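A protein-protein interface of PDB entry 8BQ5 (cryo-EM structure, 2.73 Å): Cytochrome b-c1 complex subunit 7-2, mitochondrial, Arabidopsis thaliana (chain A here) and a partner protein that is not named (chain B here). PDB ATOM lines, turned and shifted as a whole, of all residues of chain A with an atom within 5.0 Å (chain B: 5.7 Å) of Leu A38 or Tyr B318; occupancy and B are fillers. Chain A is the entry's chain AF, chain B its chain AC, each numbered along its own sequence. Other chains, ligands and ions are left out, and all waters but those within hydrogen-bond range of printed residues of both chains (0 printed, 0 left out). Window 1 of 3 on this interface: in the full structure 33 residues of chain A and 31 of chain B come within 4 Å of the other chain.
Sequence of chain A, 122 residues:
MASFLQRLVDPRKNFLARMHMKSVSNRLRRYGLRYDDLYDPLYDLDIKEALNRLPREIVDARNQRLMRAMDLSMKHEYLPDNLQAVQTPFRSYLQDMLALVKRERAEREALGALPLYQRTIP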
ATOM      1  N   LEU A  28     -25.042  33.705  13.200  1.00  0.00           N
ATOM      2  CA  LEU A  28     -23.920  33.557  12.279  1.00  0.00           C
ATOM      3  C   LEU A  28     -22.633  34.111  12.878  1.00  0.00           C
ATOM      4  O   LEU A  28     -21.559  33.523  12.713  1.00  0.00           O
ATOM      5  CB  LEU A  28     -24.235  34.256  10.959  1.00  0.00           C
ATOM      6  CG  LEU A  28     -25.199  33.536  10.019  1.00  0.00           C
ATOM      7  CD1 LEU A  28     -25.600  34.447   8.872  1.00  0.00           C
ATOM      8  CD2 LEU A  28     -24.578  32.250   9.500  1.00  0.00           C
ATOM      9  N   LEU A  33     -19.479  32.459  10.727  1.00  0.00           N
ATOM     10  CA  LEU A  33     -19.986  32.026   9.436  1.00  0.00           C
ATOM     11  C   LEU A  33     -20.648  33.180   8.700  1.00  0.00           C
ATOM     12  O   LEU A  33     -21.238  34.077   9.306  1.00  0.00           O
ATOM     13  CB  LEU A  33     -20.995  30.891   9.607  1.00  0.00           C
ATOM     14  CG  LEU A  33     -20.439  29.505   9.923  1.00  0.00           C
ATOM     15  CD1 LEU A  33     -21.576  28.537  10.179  1.00  0.00           C
ATOM     16  CD2 LEU A  33     -19.554  29.012   8.791  1.00  0.00           C
ATOM     17  N   ARG A  34     -20.535  33.151   7.380  1.00  0.00           N
ATOM     18  CA  ARG A  34     -21.316  34.026   6.528  1.00  0.00           C
ATOM     19  C   ARG A  34     -22.565  33.287   6.070  1.00  0.00           C
ATOM     20  O   ARG A  34     -22.620  32.056   6.096  1.00  0.00           O
ATOM     21  CB  ARG A  34     -20.491  34.492   5.330  1.00  0.00           C
ATOM     22  CG  ARG A  34     -19.434  35.507   5.712  1.00  0.00           C
ATOM     23  CD  ARG A  34     -18.885  36.238   4.510  1.00  0.00           C
ATOM     24  NE  ARG A  34     -17.476  36.563   4.684  1.00  0.00           N
ATOM     25  CZ  ARG A  34     -16.694  37.042   3.726  1.00  0.00           C
ATOM     26  NH1 ARG A  34     -17.154  37.263   2.507  1.00  0.00           N
ATOM     27  NH2 ARG A  34     -15.421  37.308   4.001  1.00  0.00           N
ATOM     28  N   TYR A  35     -23.582  34.051   5.669  1.00  0.00           N
ATOM     29  CA  TYR A  35     -24.833  33.427   5.257  1.00  0.00           C
ATOM     30  C   TYR A  35     -24.633  32.550   4.028  1.00  0.00           C
ATOM     31  O   TYR A  35     -25.306  31.523   3.872  1.00  0.00           O
ATOM     32  CB  TYR A  35     -25.896  34.487   4.989  1.00  0.00           C
ATOM     33  CG  TYR A  35     -27.285  33.909   4.895  1.00  0.00           C
ATOM     34  CD1 TYR A  35     -27.998  33.580   6.040  1.00  0.00           C
ATOM     35  CD2 TYR A  35     -27.878  33.674   3.664  1.00  0.00           C
ATOM     36  CE1 TYR A  35     -29.265  33.045   5.960  1.00  0.00           C
ATOM     37  CE2 TYR A  35     -29.145  33.140   3.575  1.00  0.00           C
ATOM     38  CZ  TYR A  35     -29.834  32.827   4.725  1.00  0.00           C
ATOM     39  OH  TYR A  35     -31.097  32.293   4.643  1.00  0.00           O
ATOM     40  N   ASP A  36     -23.712  32.937   3.145  1.00  0.00           N
ATOM     41  CA  ASP A  36     -23.430  32.122   1.970  1.00  0.00           C
ATOM     42  C   ASP A  36     -22.739  30.818   2.343  1.00  0.00           C
ATOM     43  O   ASP A  36     -22.821  29.840   1.591  1.00  0.00           O
ATOM     44  CB  ASP A  36     -22.580  32.912   0.981  1.00  0.00           C
ATOM     45  CG  ASP A  36     -23.386  33.935   0.219  1.00  0.00           C
ATOM     46  OD1 ASP A  36     -24.613  34.001   0.433  1.00  0.00           O
ATOM     47  OD2 ASP A  36     -22.793  34.677  -0.589  1.00  0.00           O
ATOM     48  N   ASP A  37     -22.054  30.784   3.488  1.00  0.00           N
ATOM     49  CA  ASP A  37     -21.437  29.546   3.949  1.00  0.00           C
ATOM     50  C   ASP A  37     -22.468  28.470   4.260  1.00  0.00           C
ATOM     51  O   ASP A  37     -22.130  27.282   4.240  1.00  0.00           O
ATOM     52  CB  ASP A  37     -20.577  29.807   5.186  1.00  0.00           C
ATOM     53  CG  ASP A  37     -19.380  30.686   4.892  1.00  0.00           C
ATOM     54  OD1 ASP A  37     -18.903  30.680   3.738  1.00  0.00           O
ATOM     55  OD2 ASP A  37     -18.910  31.378   5.818  1.00  0.00           O
ATOM     56  N   LEU A  38     -23.714  28.853   4.549  1.00  0.00           N
ATOM     57  CA  LEU A  38     -24.751  27.866   4.825  1.00  0.00           C
ATOM     58  C   LEU A  38     -25.180  27.115   3.573  1.00  0.00           C
ATOM     59  O   LEU A  38     -25.852  26.083   3.683  1.00  0.00           O
ATOM     60  CB  LEU A  38     -25.961  28.537   5.475  1.00  0.00           C
ATOM     61  CG  LEU A  38     -25.684  29.379   6.723  1.00  0.00           C
ATOM     62  CD1 LEU A  38     -26.969  29.946   7.297  1.00  0.00           C
ATOM     63  CD2 LEU A  38     -24.955  28.558   7.771  1.00  0.00           C
ATOM     64  N   TYR A  39     -24.885  27.676   2.399  1.00  0.00           N
ATOM     65  CA  TYR A  39     -25.290  27.052   1.114  1.00  0.00           C
ATOM     66  C   TYR A  39     -24.332  25.902   0.824  1.00  0.00           C
ATOM     67  O   TYR A  39     -23.141  26.171   0.609  1.00  0.00           O
ATOM     68  CB  TYR A  39     -25.308  28.101   0.002  1.00  0.00           C
ATOM     69  CG  TYR A  39     -26.538  28.969  -0.064  1.00  0.00           C
ATOM     70  CD1 TYR A  39     -27.081  29.546   1.072  1.00  0.00           C
ATOM     71  CD2 TYR A  39     -27.149  29.228  -1.277  1.00  0.00           C
ATOM     72  CE1 TYR A  39     -28.210  30.345   1.008  1.00  0.00           C
ATOM     73  CE2 TYR A  39     -28.274  30.029  -1.361  1.00  0.00           C
ATOM     74  CZ  TYR A  39     -28.809  30.586  -0.215  1.00  0.00           C
ATOM     75  OH  TYR A  39     -29.921  31.369  -0.294  1.00  0.00           O
ATOM     76  N   ASP A  40     -24.837  24.671   0.801  1.00  0.00           N
ATOM     77  CA  ASP A  40     -23.957  23.481   0.653  1.00  0.00           C
ATOM     78  C   ASP A  40     -24.031  22.947  -0.785  1.00  0.00           C
ATOM     79  O   ASP A  40     -25.137  22.895  -1.345  1.00  0.00           O
ATOM     80  CB  ASP A  40     -24.293  22.483   1.768  1.00  0.00           C
ATOM     81  CG  ASP A  40     -23.467  21.212   1.781  1.00  0.00           C
ATOM     82  OD1 ASP A  40     -22.257  21.315   2.007  1.00  0.00           O
ATOM     83  OD2 ASP A  40     -24.037  20.138   1.542  1.00  0.00           O
ATOM     84  N   TYR A  43     -26.551  20.086  -1.647  1.00  0.00           N
ATOM     85  CA  TYR A  43     -28.000  20.411  -1.684  1.00  0.00           C
ATOM     86  C   TYR A  43     -28.456  20.591  -3.136  1.00  0.00           C
ATOM     87  O   TYR A  43     -29.478  20.001  -3.512  1.00  0.00           O
ATOM     88  CB  TYR A  43     -28.317  21.655  -0.850  1.00  0.00           C
ATOM     89  CG  TYR A  43     -29.784  21.996  -0.819  1.00  0.00           C
ATOM     90  CD1 TYR A  43     -30.350  22.770  -1.817  1.00  0.00           C
ATOM     91  CD2 TYR A  43     -30.618  21.519   0.178  1.00  0.00           C
ATOM     92  CE1 TYR A  43     -31.700  23.060  -1.834  1.00  0.00           C
ATOM     93  CE2 TYR A  43     -31.971  21.812   0.187  1.00  0.00           C
ATOM     94  CZ  TYR A  43     -32.510  22.590  -0.822  1.00  0.00           C
ATOM     95  OH  TYR A  43     -33.832  22.907  -0.867  1.00  0.00           O
ATOM     96  N   ASP A  44     -27.745  21.408  -3.910  1.00  0.00           N
ATOM     97  CA  ASP A  44     -28.171  21.709  -5.299  1.00  0.00           C
ATOM     98  C   ASP A  44     -26.966  21.595  -6.230  1.00  0.00           C
ATOM     99  O   ASP A  44     -25.866  22.019  -5.833  1.00  0.00           O
ATOM    100  CB  ASP A  44     -28.799  23.100  -5.371  1.00  0.00           C
ATOM    101  CG  ASP A  44     -29.500  23.435  -6.676  1.00  0.00           C
ATOM    102  OD1 ASP A  44     -29.689  24.638  -6.935  1.00  0.00           O
ATOM    103  OD2 ASP A  44     -29.865  22.498  -7.413  1.00  0.00           O
ATOM    104  N   ILE A  47     -25.479  25.025  -7.033  1.00  0.00           N
ATOM    105  CA  ILE A  47     -24.536  25.570  -6.007  1.00  0.00           C
ATOM    106  C   ILE A  47     -23.145  24.999  -6.286  1.00  0.00           C
ATOM    107  O   ILE A  47     -22.194  25.778  -6.274  1.00  0.00           O
ATOM    108  CB  ILE A  47     -25.005  25.276  -4.565  1.00  0.00           C
ATOM    109  CG1 ILE A  47     -26.429  25.773  -4.308  1.00  0.00           C
ATOM    110  CG2 ILE A  47     -24.034  25.849  -3.545  1.00  0.00           C
ATOM    111  CD1 ILE A  47     -26.896  25.542  -2.893  1.00  0.00           C
ATOM    112  N   LEU A  98     -24.563  32.376  -8.258  1.00  0.00           N
ATOM    113  CA  LEU A  98     -25.667  31.423  -8.294  1.00  0.00           C
ATOM    114  C   LEU A  98     -26.785  31.904  -9.211  1.00  0.00           C
ATOM    115  O   LEU A  98     -27.399  31.105  -9.925  1.00  0.00           O
ATOM    116  CB  LEU A  98     -26.194  31.178  -6.881  1.00  0.00           C
ATOM    117  CG  LEU A  98     -27.293  30.125  -6.738  1.00  0.00           C
ATOM    118  CD1 LEU A  98     -26.807  28.777  -7.242  1.00  0.00           C
ATOM    119  CD2 LEU A  98     -27.744  30.027  -5.292  1.00  0.00           C
ATOM    120  N   LYS A 102     -28.169  29.963 -12.555  1.00  0.00           N
ATOM    121  CA  LYS A 102     -29.586  29.661 -12.727  1.00  0.00           C
ATOM    122  C   LYS A 102     -30.125  30.238 -14.031  1.00  0.00           C
ATOM    123  O   LYS A 102     -30.923  29.592 -14.719  1.00  0.00           O
ATOM    124  CB  LYS A 102     -30.385  30.183 -11.535  1.00  0.00           C
ATOM    125  CG  LYS A 102     -30.360  29.264 -10.327  1.00  0.00           C
ATOM    126  CD  LYS A 102     -30.484  30.047  -9.032  1.00  0.00           C
ATOM    127  CE  LYS A 102     -31.091  29.195  -7.930  1.00  0.00           C
ATOM    128  NZ  LYS A 102     -30.494  27.831  -7.889  1.00  0.00           N
ATOM    129  N   LEU B 216     -24.864  22.215  12.504  1.00  0.00           N
ATOM    130  CA  LEU B 216     -24.810  23.493  11.807  1.00  0.00           C
ATOM    131  C   LEU B 216     -25.472  23.442  10.435  1.00  0.00           C
ATOM    132  O   LEU B 216     -25.747  24.499   9.857  1.00  0.00           O
ATOM    133  CB  LEU B 216     -23.360  23.953  11.662  1.00  0.00           C
ATOM    134  CG  LEU B 216     -22.630  24.332  12.952  1.00  0.00           C
ATOM    135  CD1 LEU B 216     -21.177  24.652  12.661  1.00  0.00           C
ATOM    136  CD2 LEU B 216     -23.310  25.501  13.644  1.00  0.00           C
ATOM    137  N   GLY B 217     -25.727  22.248   9.904  1.00  0.00           N
ATOM    138  CA  GLY B 217     -26.367  22.107   8.611  1.00  0.00           C
ATOM    139  C   GLY B 217     -25.524  22.509   7.424  1.00  0.00           C
ATOM    140  O   GLY B 217     -26.074  22.744   6.345  1.00  0.00           O
ATOM    141  N   VAL B 218     -24.210  22.589   7.584  1.00  0.00           N
ATOM    142  CA  VAL B 218     -23.332  23.076   6.543  1.00  0.00           C
ATOM    143  C   VAL B 218     -22.540  21.913   5.959  1.00  0.00           C
ATOM    144  O   VAL B 218     -22.593  20.787   6.448  1.00  0.00           O
ATOM    145  CB  VAL B 218     -22.389  24.186   7.065  1.00  0.00           C
ATOM    146  CG1 VAL B 218     -23.191  25.343   7.626  1.00  0.00           C
ATOM    147  CG2 VAL B 218     -21.452  23.626   8.120  1.00  0.00           C
ATOM    148  N   SER B 316     -37.525  24.082  -1.123  1.00  0.00           N
ATOM    149  CA  SER B 316     -37.175  24.693   0.148  1.00  0.00           C
ATOM    150  C   SER B 316     -35.979  25.616  -0.030  1.00  0.00           C
ATOM    151  O   SER B 316     -35.319  25.624  -1.071  1.00  0.00           O
ATOM    152  CB  SER B 316     -36.855  23.627   1.198  1.00  0.00           C
ATOM    153  OG  SER B 316     -35.546  23.122   1.012  1.00  0.00           O
ATOM    154  N   MET B 317     -35.726  26.430   0.990  1.00  0.00           N
ATOM    155  CA  MET B 317     -34.539  27.261   0.968  1.00  0.00           C
ATOM    156  C   MET B 317     -33.298  26.395   1.167  1.00  0.00           C
ATOM    157  O   MET B 317     -33.375  25.204   1.482  1.00  0.00           O
ATOM    158  CB  MET B 317     -34.620  28.352   2.035  1.00  0.00           C
ATOM    159  CG  MET B 317     -34.978  27.856   3.423  1.00  0.00           C
ATOM    160  SD  MET B 317     -34.263  28.881   4.722  1.00  0.00           S
ATOM    161  CE  MET B 317     -35.629  29.983   5.077  1.00  0.00           C
ATOM    162  N   TYR B 318     -32.138  27.011   0.973  1.00  0.00           N
ATOM    163  CA  TYR B 318     -30.871  26.301   0.992  1.00  0.00           C
ATOM    164  C   TYR B 318     -30.227  26.279   2.372  1.00  0.00           C
ATOM    165  O   TYR B 318     -29.034  25.980   2.480  1.00  0.00           O
ATOM    166  CB  TYR B 318     -29.918  26.925  -0.030  1.00  0.00           C
ATOM    167  CG  TYR B 318     -30.542  27.107  -1.396  1.00  0.00           C
ATOM    168  CD1 TYR B 318     -30.414  26.131  -2.373  1.00  0.00           C
ATOM    169  CD2 TYR B 318     -31.266  28.251  -1.706  1.00  0.00           C
ATOM    170  CE1 TYR B 318     -30.983  26.290  -3.620  1.00  0.00           C
ATOM    171  CE2 TYR B 318     -31.839  28.419  -2.950  1.00  0.00           C
ATOM    172  CZ  TYR B 318     -31.694  27.435  -3.903  1.00  0.00           C
ATOM    173  OH  TYR B 318     -32.264  27.596  -5.144  1.00  0.00           O
ATOM    174  N   VAL B 319     -30.986  26.581   3.421  1.00  0.00           N
ATOM    175  CA  VAL B 319     -30.494  26.582   4.794  1.00  0.00           C
ATOM    176  C   VAL B 319     -31.217  25.481   5.555  1.00  0.00           C
ATOM    177  O   VAL B 319     -32.451  25.411   5.534  1.00  0.00           O
ATOM    178  CB  VAL B 319     -30.701  27.950   5.467  1.00  0.00           C
ATOM    179  CG1 VAL B 319     -30.144  27.936   6.879  1.00  0.00           C
ATOM    180  CG2 VAL B 319     -30.048  29.045   4.644  1.00  0.00           C
ATOM    181  N   ARG B 320     -30.449  24.623   6.226  1.00  0.00           N
ATOM    182  CA  ARG B 320     -31.004  23.428   6.852  1.00  0.00           C
ATOM    183  C   ARG B 320     -31.354  23.643   8.322  1.00  0.00           C
ATOM    184  O   ARG B 320     -32.516  23.508   8.717  1.00  0.00           O
ATOM    185  CB  ARG B 320     -30.013  22.265   6.716  1.00  0.00           C
ATOM    186  CG  ARG B 320     -29.914  21.688   5.320  1.00  0.00           C
ATOM    187  CD  ARG B 320     -29.230  20.334   5.338  1.00  0.00           C
ATOM    188  NE  ARG B 320     -28.851  19.897   4.001  1.00  0.00           N
ATOM    189  CZ  ARG B 320     -27.629  19.999   3.497  1.00  0.00           C
ATOM    190  NH1 ARG B 320     -26.634  20.515   4.198  1.00  0.00           N
ATOM    191  NH2 ARG B 320     -27.400  19.569   2.260  1.00  0.00           N
ATOM    192  N   PHE B 324     -30.307  28.495  12.531  1.00  0.00           N
ATOM    193  CA  PHE B 324     -30.179  29.695  11.712  1.00  0.00           C
ATOM    194  C   PHE B 324     -31.496  30.090  11.056  1.00  0.00           C
ATOM    195  O   PHE B 324     -31.511  31.003  10.222  1.00  0.00           O
ATOM    196  CB  PHE B 324     -29.099  29.502  10.644  1.00  0.00           C
ATOM    197  CG  PHE B 324     -27.749  29.169  11.204  1.00  0.00           C
ATOM    198  CD1 PHE B 324     -27.055  30.093  11.965  1.00  0.00           C
ATOM    199  CD2 PHE B 324     -27.176  27.931  10.974  1.00  0.00           C
ATOM    200  CE1 PHE B 324     -25.814  29.788  12.483  1.00  0.00           C
ATOM    201  CE2 PHE B 324     -25.935  27.621  11.488  1.00  0.00           C
ATOM    202  CZ  PHE B 324     -25.253  28.550  12.244  1.00  0.00           C
ATOM    203  N   ARG B 380     -36.117  32.131   0.276  1.00  0.00           N
ATOM    204  CA  ARG B 380     -35.124  32.102  -0.792  1.00  0.00           C
ATOM    205  C   ARG B 380     -34.518  33.478  -1.027  1.00  0.00           C
ATOM    206  O   ARG B 380     -33.337  33.587  -1.374  1.00  0.00           O
ATOM    207  CB  ARG B 380     -35.756  31.583  -2.083  1.00  0.00           C
ATOM    208  CG  ARG B 380     -34.814  30.783  -2.962  1.00  0.00           C
ATOM    209  CD  ARG B 380     -35.579  29.778  -3.799  1.00  0.00           C
ATOM    210  NE  ARG B 380     -36.370  28.867  -2.987  1.00  0.00           N
ATOM    211  CZ  ARG B 380     -36.254  27.549  -3.011  1.00  0.00           C
ATOM    212  NH1 ARG B 380     -35.363  26.943  -3.780  1.00  0.00           N
ATOM    213  NH2 ARG B 380     -37.069  26.819  -2.264  1.00  0.00           N
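OG of Ser B316 is in hydrogen-bond range of OH of Tyr A43, at 2.6 Å. O of Met B317 is in hydrogen-bond range of OH of Tyr A43 (3.3 Å). The side-chain amino group of Lys A102 sits at hydrogen-bond distance from the side-chain hydroxyl of Tyr B318 (3.3 Å). The guanidinium group of Arg B320 is in salt-bridge range of the side-chain carboxylate of Asp A40, 3.5 Å away. The backbone carbonyl oxygen of Tyr B318 sits close to the backbone carbonyl oxygen of Leu A38, at 3.4 Å.
The backbone carbonyl oxygen (O) of Gly B217 sits at hydrogen-bond distance from the guanidinium group (NH1) of Arg B320. O of Ser B316 lies within hydrogen-bond range of NH2 of Arg B380. The side-chain hydroxyl (OH) of Tyr B318 lies within hydrogen-bond range of the guanidinium group (NH1) of Arg B380. The side-chain amino group (NZ) of Lys A102 is in salt-bridge range of the side-chain carboxylate (OD1) of Asp A44 (3.4 Å).
Among the printed residues, pairs that only touch across the chains: Tyr A35 with Val B319 (3.4 Å), Leu A38 with Val B218 (3.7 Å), Leu A38 with Val B319 (3.8 Å), Leu A38 with Phe B324 (3.9 Å), Tyr A39 with Tyr B318 (3.5 Å), Tyr A43 with Tyr B318 (3.4 Å), Tyr A43 with Arg B320 (3.9 Å), Asp A44 with Tyr B318 (3.9 Å) and Ile A47 with Tyr B318 (3.6 Å).
Leu A38 touches just these residues of chain B: Val B218 (3.7 Å), Tyr B318 (3.4 Å), Val B319 (3.8 Å) and Phe B324 (3.9 Å). Of chain A, only Leu A38, Tyr A39, Tyr A43, Asp A44, Ile A47 and Lys A102 come within 4 Å of Tyr B318. Of the printed residues of chain A, Arg B320 touches Asp A40 and Tyr A43. Of the printed residues of chain A, Val B218 touches Leu A38. Of the printed residues of chain A, Ser B316 touches Tyr A43. The nearest residue of chain B that does not touch Leu A38 is Gly B217 (4.3 Å). The nearest printed residue of chain A that does not touch Arg B320 is Leu A38 (5.5 Å).
Hydrophobic or aromatic side chains of chain A that line the printed part of chain B: Tyr A35, Leu A38, Tyr A39, Tyr A43 and Ile A47. Among the printed residues, 14 pairs touch across the chains.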
